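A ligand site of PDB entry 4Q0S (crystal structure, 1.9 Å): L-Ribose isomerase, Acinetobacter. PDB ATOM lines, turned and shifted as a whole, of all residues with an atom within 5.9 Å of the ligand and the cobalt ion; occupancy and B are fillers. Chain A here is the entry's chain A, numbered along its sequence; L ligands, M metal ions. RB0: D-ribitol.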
ATOM      1  N   ILE A  51      -8.501 -13.647  -9.219  1.00  0.00           N
ATOM      2  CA  ILE A  51      -7.969 -13.305  -7.908  1.00  0.00           C
ATOM      3  C   ILE A  51      -6.675 -12.481  -7.924  1.00  0.00           C
ATOM      4  O   ILE A  51      -5.738 -12.777  -8.663  1.00  0.00           O
ATOM      5  CB  ILE A  51      -7.710 -14.594  -7.099  1.00  0.00           C
ATOM      6  CG1 ILE A  51      -8.988 -15.435  -7.055  1.00  0.00           C
ATOM      7  CG2 ILE A  51      -7.250 -14.263  -5.676  1.00  0.00           C
ATOM      8  CD1 ILE A  51      -8.754 -16.881  -6.610  1.00  0.00           C
ATOM      9  N   PHE A  53      -3.936 -11.184  -5.136  1.00  0.00           N
ATOM     10  CA  PHE A  53      -3.528 -11.365  -3.742  1.00  0.00           C
ATOM     11  C   PHE A  53      -2.942 -10.151  -3.036  1.00  0.00           C
ATOM     12  O   PHE A  53      -1.736 -10.101  -2.760  1.00  0.00           O
ATOM     13  CB  PHE A  53      -2.559 -12.538  -3.633  1.00  0.00           C
ATOM     14  CG  PHE A  53      -3.123 -13.852  -4.121  1.00  0.00           C
ATOM     15  CD1 PHE A  53      -3.000 -14.228  -5.460  1.00  0.00           C
ATOM     16  CD2 PHE A  53      -3.778 -14.715  -3.242  1.00  0.00           C
ATOM     17  CE1 PHE A  53      -3.510 -15.439  -5.911  1.00  0.00           C
ATOM     18  CE2 PHE A  53      -4.299 -15.927  -3.685  1.00  0.00           C
ATOM     19  CZ  PHE A  53      -4.166 -16.294  -5.020  1.00  0.00           C
ATOM     20  N   MET A  74      -4.186 -14.790 -10.072  1.00  0.00           N
ATOM     21  CA  MET A  74      -4.511 -15.969 -10.855  1.00  0.00           C
ATOM     22  C   MET A  74      -6.004 -16.082 -11.012  1.00  0.00           C
ATOM     23  O   MET A  74      -6.778 -15.338 -10.398  1.00  0.00           O
ATOM     24  CB  MET A  74      -4.019 -17.219 -10.136  1.00  0.00           C
ATOM     25  CG  MET A  74      -4.873 -17.525  -8.896  1.00  0.00           C
ATOM     26  SD  MET A  74      -4.162 -18.769  -7.823  1.00  0.00           S
ATOM     27  CE  MET A  74      -4.264 -20.210  -8.914  1.00  0.00           C
ATOM     28  N   ILE A  76      -9.272 -18.938 -11.027  1.00  0.00           N
ATOM     29  CA  ILE A  76      -9.662 -20.276 -10.618  1.00  0.00           C
ATOM     30  C   ILE A  76     -11.120 -20.479 -10.985  1.00  0.00           C
ATOM     31  O   ILE A  76     -11.968 -19.670 -10.612  1.00  0.00           O
ATOM     32  CB  ILE A  76      -9.511 -20.503  -9.098  1.00  0.00           C
ATOM     33  CG1 ILE A  76      -8.050 -20.342  -8.679  1.00  0.00           C
ATOM     34  CG2 ILE A  76     -10.021 -21.890  -8.723  1.00  0.00           C
ATOM     35  CD1 ILE A  76      -7.812 -20.499  -7.175  1.00  0.00           C
ATOM     36  N   LYS A 104     -10.897 -27.934  -9.754  1.00  0.00           N
ATOM     37  CA  LYS A 104     -10.864 -26.597 -10.326  1.00  0.00           C
ATOM     38  C   LYS A 104      -9.789 -26.492 -11.388  1.00  0.00           C
ATOM     39  O   LYS A 104      -8.880 -27.307 -11.458  1.00  0.00           O
ATOM     40  CB  LYS A 104     -10.587 -25.551  -9.236  1.00  0.00           C
ATOM     41  CG  LYS A 104      -9.144 -25.547  -8.749  1.00  0.00           C
ATOM     42  CD  LYS A 104      -9.053 -25.801  -7.240  1.00  0.00           C
ATOM     43  CE  LYS A 104      -9.533 -27.197  -6.874  1.00  0.00           C
ATOM     44  NZ  LYS A 104      -9.312 -27.534  -5.430  1.00  0.00           N
ATOM     45  N   MET A 106      -6.985 -23.849 -12.874  1.00  0.00           N
ATOM     46  CA  MET A 106      -6.279 -22.646 -12.475  1.00  0.00           C
ATOM     47  C   MET A 106      -5.476 -22.115 -13.654  1.00  0.00           C
ATOM     48  O   MET A 106      -4.794 -22.858 -14.349  1.00  0.00           O
ATOM     49  CB  MET A 106      -5.355 -22.941 -11.285  1.00  0.00           C
ATOM     50  CG  MET A 106      -6.102 -23.564 -10.120  1.00  0.00           C
ATOM     51  SD  MET A 106      -5.111 -23.773  -8.627  1.00  0.00           S
ATOM     52  CE  MET A 106      -4.000 -25.038  -9.127  1.00  0.00           C
ATOM     53  N   CYS A 114       0.881 -17.994  -7.695  1.00  0.00           N
ATOM     54  CA  CYS A 114      -0.160 -18.343  -6.742  1.00  0.00           C
ATOM     55  C   CYS A 114       0.822 -18.229  -5.563  1.00  0.00           C
ATOM     56  O   CYS A 114       1.754 -19.025  -5.441  1.00  0.00           O
ATOM     57  CB  CYS A 114      -0.624 -19.785  -6.887  1.00  0.00           C
ATOM     58  SG  CYS A 114      -1.717 -20.323  -5.516  1.00  0.00           S
ATOM     59  N   HIS A 117       1.717 -20.240   0.620  1.00  0.00           N
ATOM     60  CA  HIS A 117       0.670 -20.483   1.605  1.00  0.00           C
ATOM     61  C   HIS A 117       0.633 -21.968   1.909  1.00  0.00           C
ATOM     62  O   HIS A 117       1.318 -22.761   1.255  1.00  0.00           O
ATOM     63  CB  HIS A 117      -0.698 -20.039   1.065  1.00  0.00           C
ATOM     64  CG  HIS A 117      -1.185 -20.865  -0.095  1.00  0.00           C
ATOM     65  ND1 HIS A 117      -0.618 -20.800  -1.344  1.00  0.00           N
ATOM     66  CD2 HIS A 117      -2.148 -21.810  -0.160  1.00  0.00           C
ATOM     67  CE1 HIS A 117      -1.213 -21.667  -2.144  1.00  0.00           C
ATOM     68  NE2 HIS A 117      -2.147 -22.293  -1.452  1.00  0.00           N
ATOM     69  N   HIS A 119      -2.144 -25.184   3.773  1.00  0.00           N
ATOM     70  CA  HIS A 119      -3.473 -25.524   4.265  1.00  0.00           C
ATOM     71  C   HIS A 119      -3.377 -26.485   5.442  1.00  0.00           C
ATOM     72  O   HIS A 119      -2.561 -27.401   5.434  1.00  0.00           O
ATOM     73  CB  HIS A 119      -4.285 -26.190   3.144  1.00  0.00           C
ATOM     74  CG  HIS A 119      -4.302 -25.396   1.869  1.00  0.00           C
ATOM     75  ND1 HIS A 119      -4.997 -24.221   1.739  1.00  0.00           N
ATOM     76  CD2 HIS A 119      -3.679 -25.605   0.692  1.00  0.00           C
ATOM     77  CE1 HIS A 119      -4.798 -23.728   0.528  1.00  0.00           C
ATOM     78  NE2 HIS A 119      -4.003 -24.545  -0.130  1.00  0.00           N
ATOM     79  N   LYS A 122      -6.532 -29.078   3.686  1.00  0.00           N
ATOM     80  CA  LYS A 122      -6.522 -29.453   2.274  1.00  0.00           C
ATOM     81  C   LYS A 122      -5.238 -29.981   1.637  1.00  0.00           C
ATOM     82  O   LYS A 122      -4.191 -29.330   1.671  1.00  0.00           O
ATOM     83  CB  LYS A 122      -7.027 -28.295   1.411  1.00  0.00           C
ATOM     84  CG  LYS A 122      -7.108 -28.638  -0.087  1.00  0.00           C
ATOM     85  CD  LYS A 122      -7.720 -27.515  -0.907  1.00  0.00           C
ATOM     86  CE  LYS A 122      -6.831 -26.283  -0.924  1.00  0.00           C
ATOM     87  NZ  LYS A 122      -7.484 -25.151  -1.633  1.00  0.00           N
ATOM     88  N   GLU A 124      -3.647 -31.197  -1.943  1.00  0.00           N
ATOM     89  CA  GLU A 124      -3.845 -30.945  -3.372  1.00  0.00           C
ATOM     90  C   GLU A 124      -3.048 -31.898  -4.262  1.00  0.00           C
ATOM     91  O   GLU A 124      -2.119 -32.569  -3.807  1.00  0.00           O
ATOM     92  CB  GLU A 124      -3.426 -29.520  -3.718  1.00  0.00           C
ATOM     93  CG  GLU A 124      -4.059 -28.424  -2.862  1.00  0.00           C
ATOM     94  CD  GLU A 124      -3.387 -27.054  -3.048  1.00  0.00           C
ATOM     95  OE1 GLU A 124      -2.463 -26.921  -3.874  1.00  0.00           O
ATOM     96  OE2 GLU A 124      -3.793 -26.099  -2.350  1.00  0.00           O
ATOM     97  N   TYR A 126      -1.722 -31.844  -8.605  1.00  0.00           N
ATOM     98  CA  TYR A 126      -1.674 -31.028  -9.807  1.00  0.00           C
ATOM     99  C   TYR A 126      -1.532 -31.805 -11.093  1.00  0.00           C
ATOM    100  O   TYR A 126      -0.805 -32.795 -11.167  1.00  0.00           O
ATOM    101  CB  TYR A 126      -0.517 -30.031  -9.740  1.00  0.00           C
ATOM    102  CG  TYR A 126      -0.380 -29.280  -8.440  1.00  0.00           C
ATOM    103  CD1 TYR A 126      -1.464 -28.598  -7.903  1.00  0.00           C
ATOM    104  CD2 TYR A 126       0.835 -29.256  -7.757  1.00  0.00           C
ATOM    105  CE1 TYR A 126      -1.350 -27.895  -6.707  1.00  0.00           C
ATOM    106  CE2 TYR A 126       0.967 -28.565  -6.562  1.00  0.00           C
ATOM    107  CZ  TYR A 126      -0.125 -27.889  -6.038  1.00  0.00           C
ATOM    108  OH  TYR A 126      -0.015 -27.218  -4.839  1.00  0.00           O
ATOM    109  N   HIS A 199       3.508 -23.956  -0.047  1.00  0.00           N
ATOM    110  CA  HIS A 199       3.667 -24.088  -1.485  1.00  0.00           C
ATOM    111  C   HIS A 199       3.247 -22.836  -2.227  1.00  0.00           C
ATOM    112  O   HIS A 199       2.488 -22.009  -1.717  1.00  0.00           O
ATOM    113  CB  HIS A 199       2.902 -25.311  -2.018  1.00  0.00           C
ATOM    114  CG  HIS A 199       1.437 -25.284  -1.731  1.00  0.00           C
ATOM    115  ND1 HIS A 199       0.908 -25.527  -0.473  1.00  0.00           N
ATOM    116  CD2 HIS A 199       0.374 -25.014  -2.531  1.00  0.00           C
ATOM    117  CE1 HIS A 199      -0.400 -25.418  -0.512  1.00  0.00           C
ATOM    118  NE2 HIS A 199      -0.754 -25.108  -1.750  1.00  0.00           N
ATOM    119  N   PHE A 201       3.432 -21.415  -6.739  1.00  0.00           N
ATOM    120  CA  PHE A 201       3.776 -21.810  -8.088  1.00  0.00           C
ATOM    121  C   PHE A 201       3.574 -20.662  -9.063  1.00  0.00           C
ATOM    122  O   PHE A 201       2.794 -19.749  -8.805  1.00  0.00           O
ATOM    123  CB  PHE A 201       2.979 -23.046  -8.503  1.00  0.00           C
ATOM    124  CG  PHE A 201       1.474 -22.878  -8.438  1.00  0.00           C
ATOM    125  CD1 PHE A 201       0.778 -22.259  -9.465  1.00  0.00           C
ATOM    126  CD2 PHE A 201       0.762 -23.374  -7.346  1.00  0.00           C
ATOM    127  CE1 PHE A 201      -0.618 -22.143  -9.419  1.00  0.00           C
ATOM    128  CE2 PHE A 201      -0.635 -23.260  -7.290  1.00  0.00           C
ATOM    129  CZ  PHE A 201      -1.320 -22.650  -8.328  1.00  0.00           C
ATOM    130  N   GLU A 215      -6.624 -28.823 -10.734  1.00  0.00           N
ATOM    131  CA  GLU A 215      -6.350 -29.222  -9.349  1.00  0.00           C
ATOM    132  C   GLU A 215      -7.456 -30.112  -8.823  1.00  0.00           C
ATOM    133  O   GLU A 215      -8.642 -29.805  -8.950  1.00  0.00           O
ATOM    134  CB  GLU A 215      -6.217 -28.002  -8.424  1.00  0.00           C
ATOM    135  CG  GLU A 215      -6.012 -28.416  -6.957  1.00  0.00           C
ATOM    136  CD  GLU A 215      -5.944 -27.237  -6.016  1.00  0.00           C
ATOM    137  OE1 GLU A 215      -4.985 -26.449  -6.128  1.00  0.00           O
ATOM    138  OE2 GLU A 215      -6.843 -27.103  -5.152  1.00  0.00           O
ATOM    139  N   SER A 220     -12.455 -27.475  -0.216  1.00  0.00           N
ATOM    140  CA  SER A 220     -11.867 -26.149  -0.081  1.00  0.00           C
ATOM    141  C   SER A 220     -12.714 -25.276   0.859  1.00  0.00           C
ATOM    142  O   SER A 220     -13.810 -24.845   0.510  1.00  0.00           O
ATOM    143  CB  SER A 220     -11.752 -25.494  -1.453  1.00  0.00           C
ATOM    144  OG  SER A 220     -11.063 -24.262  -1.379  1.00  0.00           O
ATOM    145  N   GLU A 222     -13.344 -21.999   2.138  1.00  0.00           N
ATOM    146  CA  GLU A 222     -13.052 -20.599   1.844  1.00  0.00           C
ATOM    147  C   GLU A 222     -14.302 -19.721   1.838  1.00  0.00           C
ATOM    148  O   GLU A 222     -15.078 -19.749   0.884  1.00  0.00           O
ATOM    149  CB  GLU A 222     -12.360 -20.475   0.487  1.00  0.00           C
ATOM    150  CG  GLU A 222     -11.039 -21.208   0.377  1.00  0.00           C
ATOM    151  CD  GLU A 222     -10.436 -21.114  -1.016  1.00  0.00           C
ATOM    152  OE1 GLU A 222     -11.124 -21.501  -1.984  1.00  0.00           O
ATOM    153  OE2 GLU A 222      -9.277 -20.651  -1.132  1.00  0.00           O
ATOM    154  N   ASN A 243      -6.922 -21.306   4.619  1.00  0.00           N
ATOM    155  CA  ASN A 243      -5.858 -20.703   3.813  1.00  0.00           C
ATOM    156  C   ASN A 243      -4.958 -19.909   4.744  1.00  0.00           C
ATOM    157  O   ASN A 243      -5.428 -19.066   5.504  1.00  0.00           O
ATOM    158  CB  ASN A 243      -6.418 -19.755   2.746  1.00  0.00           C
ATOM    159  CG  ASN A 243      -7.135 -20.488   1.632  1.00  0.00           C
ATOM    160  OD1 ASN A 243      -6.865 -21.662   1.367  1.00  0.00           O
ATOM    161  ND2 ASN A 243      -8.041 -19.791   0.958  1.00  0.00           N
ATOM    162  N   PHE A 245      -1.707 -17.750   4.141  1.00  0.00           N
ATOM    163  CA  PHE A 245      -0.690 -17.165   3.285  1.00  0.00           C
ATOM    164  C   PHE A 245       0.454 -16.627   4.117  1.00  0.00           C
ATOM    165  O   PHE A 245       0.237 -16.068   5.196  1.00  0.00           O
ATOM    166  CB  PHE A 245      -1.310 -16.046   2.442  1.00  0.00           C
ATOM    167  CG  PHE A 245      -2.292 -16.541   1.420  1.00  0.00           C
ATOM    168  CD1 PHE A 245      -1.869 -16.881   0.133  1.00  0.00           C
ATOM    169  CD2 PHE A 245      -3.635 -16.733   1.747  1.00  0.00           C
ATOM    170  CE1 PHE A 245      -2.762 -17.410  -0.794  1.00  0.00           C
ATOM    171  CE2 PHE A 245      -4.539 -17.264   0.829  1.00  0.00           C
ATOM    172  CZ  PHE A 245      -4.097 -17.607  -0.447  1.00  0.00           C
ATOM    173  N   ARG A 254      -7.458 -12.039  -1.026  1.00  0.00           N
ATOM    174  CA  ARG A 254      -7.814 -13.339  -1.571  1.00  0.00           C
ATOM    175  C   ARG A 254      -9.326 -13.524  -1.672  1.00  0.00           C
ATOM    176  O   ARG A 254      -9.841 -13.967  -2.704  1.00  0.00           O
ATOM    177  CB  ARG A 254      -7.207 -14.445  -0.686  1.00  0.00           C
ATOM    178  CG  ARG A 254      -7.018 -15.791  -1.376  1.00  0.00           C
ATOM    179  CD  ARG A 254      -8.329 -16.391  -1.881  1.00  0.00           C
ATOM    180  NE  ARG A 254      -8.133 -17.689  -2.508  1.00  0.00           N
ATOM    181  CZ  ARG A 254      -9.089 -18.388  -3.107  1.00  0.00           C
ATOM    182  NH1 ARG A 254      -8.813 -19.565  -3.650  1.00  0.00           N
ATOM    183  NH2 ARG A 254     -10.330 -17.909  -3.165  1.00  0.00           N
HETATM  184  C1  RB0 L   1      -5.223 -20.724  -3.980  1.00  0.00           C
HETATM  185  O1  RB0 L   1      -5.790 -19.477  -3.609  1.00  0.00           O
HETATM  186  C2  RB0 L   1      -6.317 -21.780  -4.021  1.00  0.00           C
HETATM  187  O2  RB0 L   1      -6.717 -22.115  -2.696  1.00  0.00           O
HETATM  188  C3  RB0 L   1      -5.823 -23.033  -4.782  1.00  0.00           C
HETATM  189  O3  RB0 L   1      -6.917 -23.916  -5.013  1.00  0.00           O
HETATM  190  C4  RB0 L   1      -4.704 -23.781  -4.054  1.00  0.00           C
HETATM  191  O4  RB0 L   1      -4.714 -23.441  -2.670  1.00  0.00           O
HETATM  192  C5  RB0 L   1      -3.354 -23.427  -4.665  1.00  0.00           C
HETATM  193  O5  RB0 L   1      -2.335 -24.250  -4.097  1.00  0.00           O
HETATM  194 CO    CO M   1      -2.948 -24.390  -2.005  1.00  0.00          CO
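NH1 of Arg 254 sits at hydrogen-bond distance from O1 of the ligand (3.0 Å). OE2 of Glu 215 is in hydrogen-bond range of O3 of the ligand (3.2 Å). The side-chain amino group (NZ) of Lys 122 is in hydrogen-bond range of an oxygen (O2) of the ligand (3.3 Å). OE2 of Glu 222 sits at hydrogen-bond distance from O2 of the ligand (3.3 Å).
Phe 53 touches the ligand (CZ to O1, 3.8 Å). Ile 76 touches the ligand (CD1 to C2, 3.7 Å). CD of Lys 104 touches O3 of the ligand, at 3.6 Å. Met 106 touches the ligand. Cys 114 touches the ligand. Tyr 126 touches the ligand (OH to O5, 3.8 Å). Phe 201 touches the ligand. Hydrophobic or aromatic side chains within 4 Å of the ligand: Phe 53, Ile 76, Met 106, His 117, His 119, His 199 and Phe 201. Within 4 Å of the ligand: Phe 53, Ile 76, Lys 104, Met 106, Cys 114, His 117, His 119, Lys 122, Glu 124, Tyr 126, His 199, Phe 201, Glu 215, Glu 222 and Arg 254.
The cobalt ion is bound by OE2 of Glu 124 (1.9 Å), O4 of the ligand (2.1 Å), NE2 of His 119 (2.2 Å), O5 of the ligand (2.2 Å), NE2 of His 117 (2.3 Å) and NE2 of His 199 (2.3 Å).
OE2 of Glu 124 lies close to NZ of Lys 122 (3.9 Å). OH of Tyr 126 sits at hydrogen-bond distance from OE1 of Glu 124 (2.6 Å). A ring nitrogen (ND1) of His 119 sits close to the side-chain amide oxygen (OD1) of Asn 243 (3.2 Å). The guanidinium group (NH1) of Arg 254 lies within salt-bridge range of the side-chain carboxylate (OE2) of Glu 222 (2.8 Å). The side-chain carboxylate (OE2) of Glu 215 is in salt-bridge range of the side-chain amino group (NZ) of Lys 104, at 2.5 Å. The side-chain hydroxyl (OG) of Ser 220 sits at hydrogen-bond distance from the side-chain carboxylate (OE1) of Glu 222 (2.8 Å). The backbone NH (N) of Cys 114 is in hydrogen-bond range of the backbone carbonyl oxygen (O) of Phe 201. The side-chain sulfur (SG) of Cys 114 is in hydrogen-bond range of the side-chain sulfur (SD) of Met 74.
Of the 20 residues printed, 4 come within 4 Å of the cobalt ion.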
